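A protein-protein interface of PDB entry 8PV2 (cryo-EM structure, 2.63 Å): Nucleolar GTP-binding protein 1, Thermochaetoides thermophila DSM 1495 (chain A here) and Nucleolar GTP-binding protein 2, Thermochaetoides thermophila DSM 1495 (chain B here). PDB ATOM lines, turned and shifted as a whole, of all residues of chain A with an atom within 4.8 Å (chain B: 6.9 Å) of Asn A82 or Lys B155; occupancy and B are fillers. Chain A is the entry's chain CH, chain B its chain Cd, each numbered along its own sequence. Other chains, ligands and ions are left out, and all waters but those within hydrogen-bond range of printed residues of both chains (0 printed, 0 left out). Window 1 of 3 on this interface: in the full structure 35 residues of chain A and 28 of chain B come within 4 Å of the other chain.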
ATOM      1  N   ARG A  78       3.353 -23.020 -25.760  1.00  0.00           N
ATOM      2  CA  ARG A  78       1.991 -22.854 -25.260  1.00  0.00           C
ATOM      3  C   ARG A  78       1.962 -22.019 -23.986  1.00  0.00           C
ATOM      4  O   ARG A  78       1.156 -21.085 -23.857  1.00  0.00           O
ATOM      5  CB  ARG A  78       1.361 -24.224 -25.021  1.00  0.00           C
ATOM      6  CG  ARG A  78       0.007 -24.184 -24.352  1.00  0.00           C
ATOM      7  CD  ARG A  78      -0.400 -25.557 -23.871  1.00  0.00           C
ATOM      8  NE  ARG A  78      -0.008 -26.591 -24.820  1.00  0.00           N
ATOM      9  CZ  ARG A  78       0.570 -27.737 -24.488  1.00  0.00           C
ATOM     10  NH1 ARG A  78       0.844 -28.034 -23.228  1.00  0.00           N
ATOM     11  NH2 ARG A  78       0.879 -28.609 -25.443  1.00  0.00           N
ATOM     12  N   ASP A  79       2.868 -22.302 -23.053  1.00  0.00           N
ATOM     13  CA  ASP A  79       2.865 -21.547 -21.809  1.00  0.00           C
ATOM     14  C   ASP A  79       3.424 -20.143 -22.005  1.00  0.00           C
ATOM     15  O   ASP A  79       2.995 -19.209 -21.322  1.00  0.00           O
ATOM     16  CB  ASP A  79       3.624 -22.317 -20.736  1.00  0.00           C
ATOM     17  CG  ASP A  79       2.833 -23.502 -20.222  1.00  0.00           C
ATOM     18  OD1 ASP A  79       1.742 -23.282 -19.656  1.00  0.00           O
ATOM     19  OD2 ASP A  79       3.286 -24.651 -20.391  1.00  0.00           O
ATOM     20  N   LEU A  80       4.340 -19.959 -22.959  1.00  0.00           N
ATOM     21  CA  LEU A  80       4.813 -18.614 -23.270  1.00  0.00           C
ATOM     22  C   LEU A  80       3.714 -17.769 -23.895  1.00  0.00           C
ATOM     23  O   LEU A  80       3.596 -16.575 -23.598  1.00  0.00           O
ATOM     24  CB  LEU A  80       6.021 -18.681 -24.200  1.00  0.00           C
ATOM     25  CG  LEU A  80       6.655 -17.334 -24.558  1.00  0.00           C
ATOM     26  CD1 LEU A  80       7.108 -16.594 -23.315  1.00  0.00           C
ATOM     27  CD2 LEU A  80       7.804 -17.517 -25.525  1.00  0.00           C
ATOM     28  N   MET A  81       2.913 -18.361 -24.780  1.00  0.00           N
ATOM     29  CA  MET A  81       1.800 -17.624 -25.365  1.00  0.00           C
ATOM     30  C   MET A  81       0.738 -17.313 -24.324  1.00  0.00           C
ATOM     31  O   MET A  81       0.076 -16.272 -24.401  1.00  0.00           O
ATOM     32  CB  MET A  81       1.210 -18.399 -26.541  1.00  0.00           C
ATOM     33  CG  MET A  81       2.148 -18.497 -27.724  1.00  0.00           C
ATOM     34  SD  MET A  81       1.459 -19.416 -29.102  1.00  0.00           S
ATOM     35  CE  MET A  81       2.844 -19.407 -30.232  1.00  0.00           C
ATOM     36  N   ASN A  82       0.567 -18.192 -23.333  1.00  0.00           N
ATOM     37  CA  ASN A  82      -0.286 -17.850 -22.199  1.00  0.00           C
ATOM     38  C   ASN A  82       0.274 -16.673 -21.406  1.00  0.00           C
ATOM     39  O   ASN A  82      -0.476 -15.773 -21.012  1.00  0.00           O
ATOM     40  CB  ASN A  82      -0.463 -19.054 -21.282  1.00  0.00           C
ATOM     41  CG  ASN A  82      -1.109 -18.683 -19.967  1.00  0.00           C
ATOM     42  OD1 ASN A  82      -2.223 -18.170 -19.934  1.00  0.00           O
ATOM     43  ND2 ASN A  82      -0.406 -18.928 -18.874  1.00  0.00           N
ATOM     44  N   ILE A  83       1.584 -16.671 -21.153  1.00  0.00           N
ATOM     45  CA  ILE A  83       2.203 -15.604 -20.367  1.00  0.00           C
ATOM     46  C   ILE A  83       2.081 -14.269 -21.089  1.00  0.00           C
ATOM     47  O   ILE A  83       1.751 -13.244 -20.483  1.00  0.00           O
ATOM     48  CB  ILE A  83       3.674 -15.952 -20.060  1.00  0.00           C
ATOM     49  CG1 ILE A  83       3.756 -17.108 -19.066  1.00  0.00           C
ATOM     50  CG2 ILE A  83       4.428 -14.757 -19.528  1.00  0.00           C
ATOM     51  CD1 ILE A  83       3.104 -16.831 -17.752  1.00  0.00           C
ATOM     52  N   LEU A  84       2.322 -14.265 -22.397  1.00  0.00           N
ATOM     53  CA  LEU A  84       2.282 -13.022 -23.153  1.00  0.00           C
ATOM     54  C   LEU A  84       0.859 -12.539 -23.409  1.00  0.00           C
ATOM     55  O   LEU A  84       0.582 -11.344 -23.271  1.00  0.00           O
ATOM     56  CB  LEU A  84       3.027 -13.192 -24.472  1.00  0.00           C
ATOM     57  CG  LEU A  84       4.522 -13.474 -24.350  1.00  0.00           C
ATOM     58  CD1 LEU A  84       5.105 -13.820 -25.705  1.00  0.00           C
ATOM     59  CD2 LEU A  84       5.240 -12.294 -23.730  1.00  0.00           C
ATOM     60  N   TYR A  85      -0.061 -13.435 -23.779  1.00  0.00           N
ATOM     61  CA  TYR A  85      -1.323 -13.003 -24.358  1.00  0.00           C
ATOM     62  C   TYR A  85      -2.579 -13.436 -23.620  1.00  0.00           C
ATOM     63  O   TYR A  85      -3.669 -13.141 -24.121  1.00  0.00           O
ATOM     64  CB  TYR A  85      -1.449 -13.497 -25.808  1.00  0.00           C
ATOM     65  CG  TYR A  85      -0.240 -13.263 -26.674  1.00  0.00           C
ATOM     66  CD1 TYR A  85       0.199 -11.980 -26.952  1.00  0.00           C
ATOM     67  CD2 TYR A  85       0.452 -14.329 -27.235  1.00  0.00           C
ATOM     68  CE1 TYR A  85       1.297 -11.765 -27.747  1.00  0.00           C
ATOM     69  CE2 TYR A  85       1.552 -14.123 -28.031  1.00  0.00           C
ATOM     70  CZ  TYR A  85       1.969 -12.837 -28.284  1.00  0.00           C
ATOM     71  OH  TYR A  85       3.067 -12.619 -29.079  1.00  0.00           O
ATOM     72  N   ASP A  86      -2.474 -14.114 -22.467  1.00  0.00           N
ATOM     73  CA  ASP A  86      -3.635 -14.623 -21.729  1.00  0.00           C
ATOM     74  C   ASP A  86      -4.472 -15.589 -22.563  1.00  0.00           C
ATOM     75  O   ASP A  86      -5.437 -15.172 -23.216  1.00  0.00           O
ATOM     76  CB  ASP A  86      -4.517 -13.503 -21.172  1.00  0.00           C
ATOM     77  CG  ASP A  86      -5.539 -14.015 -20.175  1.00  0.00           C
ATOM     78  OD1 ASP A  86      -5.354 -15.124 -19.637  1.00  0.00           O
ATOM     79  OD2 ASP A  86      -6.528 -13.305 -19.920  1.00  0.00           O
ATOM     80  N   ALA A  87      -4.011 -16.846 -22.625  1.00  0.00           N
ATOM     81  CA  ALA A  87      -4.646 -17.931 -23.384  1.00  0.00           C
ATOM     82  C   ALA A  87      -6.174 -17.940 -23.297  1.00  0.00           C
ATOM     83  O   ALA A  87      -6.843 -18.285 -24.277  1.00  0.00           O
ATOM     84  CB  ALA A  87      -4.095 -19.270 -22.902  1.00  0.00           C
ATOM     85  N   ASP A  88      -6.745 -17.574 -22.144  1.00  0.00           N
ATOM     86  CA  ASP A  88      -8.199 -17.448 -22.032  1.00  0.00           C
ATOM     87  C   ASP A  88      -8.751 -16.414 -23.006  1.00  0.00           C
ATOM     88  O   ASP A  88      -9.670 -16.706 -23.780  1.00  0.00           O
ATOM     89  CB  ASP A  88      -8.584 -17.075 -20.601  1.00  0.00           C
ATOM     90  CG  ASP A  88      -8.584 -18.262 -19.664  1.00  0.00           C
ATOM     91  OD1 ASP A  88      -8.812 -19.396 -20.130  1.00  0.00           O
ATOM     92  OD2 ASP A  88      -8.361 -18.054 -18.454  1.00  0.00           O
ATOM     93  N   ARG B 138     -14.841  -9.621 -16.524  1.00  0.00           N
ATOM     94  CA  ARG B 138     -13.815  -9.396 -15.511  1.00  0.00           C
ATOM     95  C   ARG B 138     -12.635  -8.619 -16.077  1.00  0.00           C
ATOM     96  O   ARG B 138     -12.180  -7.644 -15.471  1.00  0.00           O
ATOM     97  CB  ARG B 138     -13.351 -10.730 -14.935  1.00  0.00           C
ATOM     98  CG  ARG B 138     -12.359 -10.604 -13.798  1.00  0.00           C
ATOM     99  CD  ARG B 138     -11.663 -11.925 -13.491  1.00  0.00           C
ATOM    100  NE  ARG B 138     -12.566 -13.068 -13.539  1.00  0.00           N
ATOM    101  CZ  ARG B 138     -12.510 -14.031 -14.449  1.00  0.00           C
ATOM    102  NH1 ARG B 138     -11.593 -14.029 -15.401  1.00  0.00           N
ATOM    103  NH2 ARG B 138     -13.397 -15.019 -14.401  1.00  0.00           N
ATOM    104  N   GLU B 139     -12.123  -9.034 -17.233  1.00  0.00           N
ATOM    105  CA  GLU B 139     -10.986  -8.379 -17.875  1.00  0.00           C
ATOM    106  C   GLU B 139     -11.345  -8.093 -19.326  1.00  0.00           C
ATOM    107  O   GLU B 139     -11.514  -9.034 -20.120  1.00  0.00           O
ATOM    108  CB  GLU B 139      -9.739  -9.250 -17.796  1.00  0.00           C
ATOM    109  CG  GLU B 139      -9.432  -9.792 -16.415  1.00  0.00           C
ATOM    110  CD  GLU B 139      -8.661 -11.093 -16.457  1.00  0.00           C
ATOM    111  OE1 GLU B 139      -9.081 -12.052 -15.780  1.00  0.00           O
ATOM    112  OE2 GLU B 139      -7.635 -11.159 -17.165  1.00  0.00           O
ATOM    113  N   ARG B 151      -2.514  -5.506 -17.610  1.00  0.00           N
ATOM    114  CA  ARG B 151      -2.311  -6.828 -17.038  1.00  0.00           C
ATOM    115  C   ARG B 151      -0.860  -7.007 -16.609  1.00  0.00           C
ATOM    116  O   ARG B 151       0.061  -6.809 -17.406  1.00  0.00           O
ATOM    117  CB  ARG B 151      -2.705  -7.890 -18.059  1.00  0.00           C
ATOM    118  CG  ARG B 151      -2.222  -9.287 -17.761  1.00  0.00           C
ATOM    119  CD  ARG B 151      -2.727 -10.236 -18.824  1.00  0.00           C
ATOM    120  NE  ARG B 151      -2.220 -11.591 -18.655  1.00  0.00           N
ATOM    121  CZ  ARG B 151      -1.170 -12.079 -19.299  1.00  0.00           C
ATOM    122  NH1 ARG B 151      -0.476 -11.342 -20.144  1.00  0.00           N
ATOM    123  NH2 ARG B 151      -0.811 -13.340 -19.086  1.00  0.00           N
ATOM    124  N   ARG B 153       0.065  -9.584 -13.533  1.00  0.00           N
ATOM    125  CA  ARG B 153       0.269 -10.972 -13.139  1.00  0.00           C
ATOM    126  C   ARG B 153      -0.493 -11.897 -14.066  1.00  0.00           C
ATOM    127  O   ARG B 153      -1.681 -11.664 -14.326  1.00  0.00           O
ATOM    128  CB  ARG B 153      -0.177 -11.211 -11.699  1.00  0.00           C
ATOM    129  CG  ARG B 153       0.836 -10.803 -10.650  1.00  0.00           C
ATOM    130  CD  ARG B 153       0.651  -9.374 -10.211  1.00  0.00           C
ATOM    131  NE  ARG B 153       1.495  -9.054  -9.067  1.00  0.00           N
ATOM    132  CZ  ARG B 153       2.692  -8.492  -9.159  1.00  0.00           C
ATOM    133  NH1 ARG B 153       3.210  -8.160 -10.329  1.00  0.00           N
ATOM    134  NH2 ARG B 153       3.382  -8.251  -8.050  1.00  0.00           N
ATOM    135  N   PRO B 154       0.141 -12.941 -14.586  1.00  0.00           N
ATOM    136  CA  PRO B 154      -0.572 -13.907 -15.421  1.00  0.00           C
ATOM    137  C   PRO B 154      -1.418 -14.848 -14.575  1.00  0.00           C
ATOM    138  O   PRO B 154      -1.357 -14.858 -13.348  1.00  0.00           O
ATOM    139  CB  PRO B 154       0.561 -14.659 -16.119  1.00  0.00           C
ATOM    140  CG  PRO B 154       1.665 -14.611 -15.139  1.00  0.00           C
ATOM    141  CD  PRO B 154       1.564 -13.288 -14.441  1.00  0.00           C
ATOM    142  N   LYS B 155      -2.224 -15.647 -15.265  1.00  0.00           N
ATOM    143  CA  LYS B 155      -3.019 -16.689 -14.634  1.00  0.00           C
ATOM    144  C   LYS B 155      -2.284 -18.013 -14.782  1.00  0.00           C
ATOM    145  O   LYS B 155      -1.957 -18.424 -15.898  1.00  0.00           O
ATOM    146  CB  LYS B 155      -4.410 -16.767 -15.260  1.00  0.00           C
ATOM    147  CG  LYS B 155      -5.163 -18.040 -14.933  1.00  0.00           C
ATOM    148  CD  LYS B 155      -6.660 -17.826 -15.019  1.00  0.00           C
ATOM    149  CE  LYS B 155      -7.379 -19.125 -15.327  1.00  0.00           C
ATOM    150  NZ  LYS B 155      -6.831 -20.258 -14.535  1.00  0.00           N
ATOM    151  N   LEU B 156      -2.024 -18.673 -13.660  1.00  0.00           N
ATOM    152  CA  LEU B 156      -1.241 -19.897 -13.635  1.00  0.00           C
ATOM    153  C   LEU B 156      -2.066 -21.044 -13.067  1.00  0.00           C
ATOM    154  O   LEU B 156      -2.870 -20.867 -12.150  1.00  0.00           O
ATOM    155  CB  LEU B 156       0.032 -19.716 -12.803  1.00  0.00           C
ATOM    156  CG  LEU B 156       0.892 -18.497 -13.133  1.00  0.00           C
ATOM    157  CD1 LEU B 156       2.009 -18.352 -12.125  1.00  0.00           C
ATOM    158  CD2 LEU B 156       1.449 -18.603 -14.534  1.00  0.00           C
ATOM    159  N   SER B 157      -1.846 -22.232 -13.623  1.00  0.00           N
ATOM    160  CA  SER B 157      -2.450 -23.459 -13.125  1.00  0.00           C
ATOM    161  C   SER B 157      -1.585 -24.139 -12.074  1.00  0.00           C
ATOM    162  O   SER B 157      -1.899 -25.252 -11.646  1.00  0.00           O
ATOM    163  CB  SER B 157      -2.728 -24.418 -14.282  1.00  0.00           C
ATOM    164  OG  SER B 157      -1.527 -24.827 -14.905  1.00  0.00           O
ATOM    165  N   PHE B 158      -0.504 -23.490 -11.655  1.00  0.00           N
ATOM    166  CA  PHE B 158       0.408 -24.009 -10.651  1.00  0.00           C
ATOM    167  C   PHE B 158       0.682 -22.900  -9.647  1.00  0.00           C
ATOM    168  O   PHE B 158       0.539 -21.715  -9.952  1.00  0.00           O
ATOM    169  CB  PHE B 158       1.716 -24.508 -11.281  1.00  0.00           C
ATOM    170  CG  PHE B 158       2.283 -23.575 -12.313  1.00  0.00           C
ATOM    171  CD1 PHE B 158       3.132 -22.548 -11.942  1.00  0.00           C
ATOM    172  CD2 PHE B 158       1.969 -23.726 -13.653  1.00  0.00           C
ATOM    173  CE1 PHE B 158       3.648 -21.684 -12.884  1.00  0.00           C
ATOM    174  CE2 PHE B 158       2.482 -22.864 -14.598  1.00  0.00           C
ATOM    175  CZ  PHE B 158       3.320 -21.841 -14.212  1.00  0.00           C
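The guanidinium group (NH1) of Arg B151 is in hydrogen-bond range of the backbone carbonyl oxygen (O) of Leu A84.
The guanidinium group (NH2) of Arg B151 sits at hydrogen-bond distance from the backbone carbonyl oxygen (O) of Ile A83 (2.9 Å).
ND2 of Asn A82 sits at hydrogen-bond distance from O of Lys B155 (3.4 Å).
The backbone carbonyl oxygen (O) of Asn A82 lies within hydrogen-bond range of the guanidinium group (NH2) of Arg B151 (3.1 Å).
NH1 of Arg B138 lies within salt-bridge range of OE1 of Glu B139, 3.2 Å away.
The backbone NH (N) of Ala A87 lies within hydrogen-bond range of the side-chain amide oxygen (OD1) of Asn A82 (3.5 Å).
CD1 of Ile A83 touches CG of Pro B154, at 3.7 Å.
Asp A86 touches Glu B139.
N of Asp A86 touches NH2 of Arg B151 (3.8 Å).
Asp A88 touches Lys B155 (OD2 to CE, 3.4 Å).
Of the printed residues of chain B, Asp A86 touches Glu B139 (3.7 Å) and Arg B151 (3.8 Å).
Printed residues of chain A within 4 Å of Pro B154: Ile A83.
Of chain A, only Asn A82 (3.4 Å) and Asp A88 (3.4 Å) come within 4 Å of Lys B155.
Leu B156 touches none of the printed residues of chain A.
The nearest printed residue of chain A that does not touch Lys B155 is Asp A86 (4.8 Å).
The nearest printed residue of chain B that does not touch Asp A88 is Arg B138 (6.0 Å).
Of the 9 printed residues of chain B, 4 touch a printed residue of chain A.
Hydrophobic or aromatic side chains of chain B that line the printed part of chain A: Pro B154.
Of the 11 printed residues of chain A, 5 touch a printed residue of chain B.
Along chain A the printed residues that touch a printed residue of chain B span positions 82 to 88.
Among the printed residues, 8 pairs touch across the chains.
Among the printed residues, no Asp or Glu carboxylate lies within 4 Å of a Lys or Arg side-chain nitrogen of the other chain.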
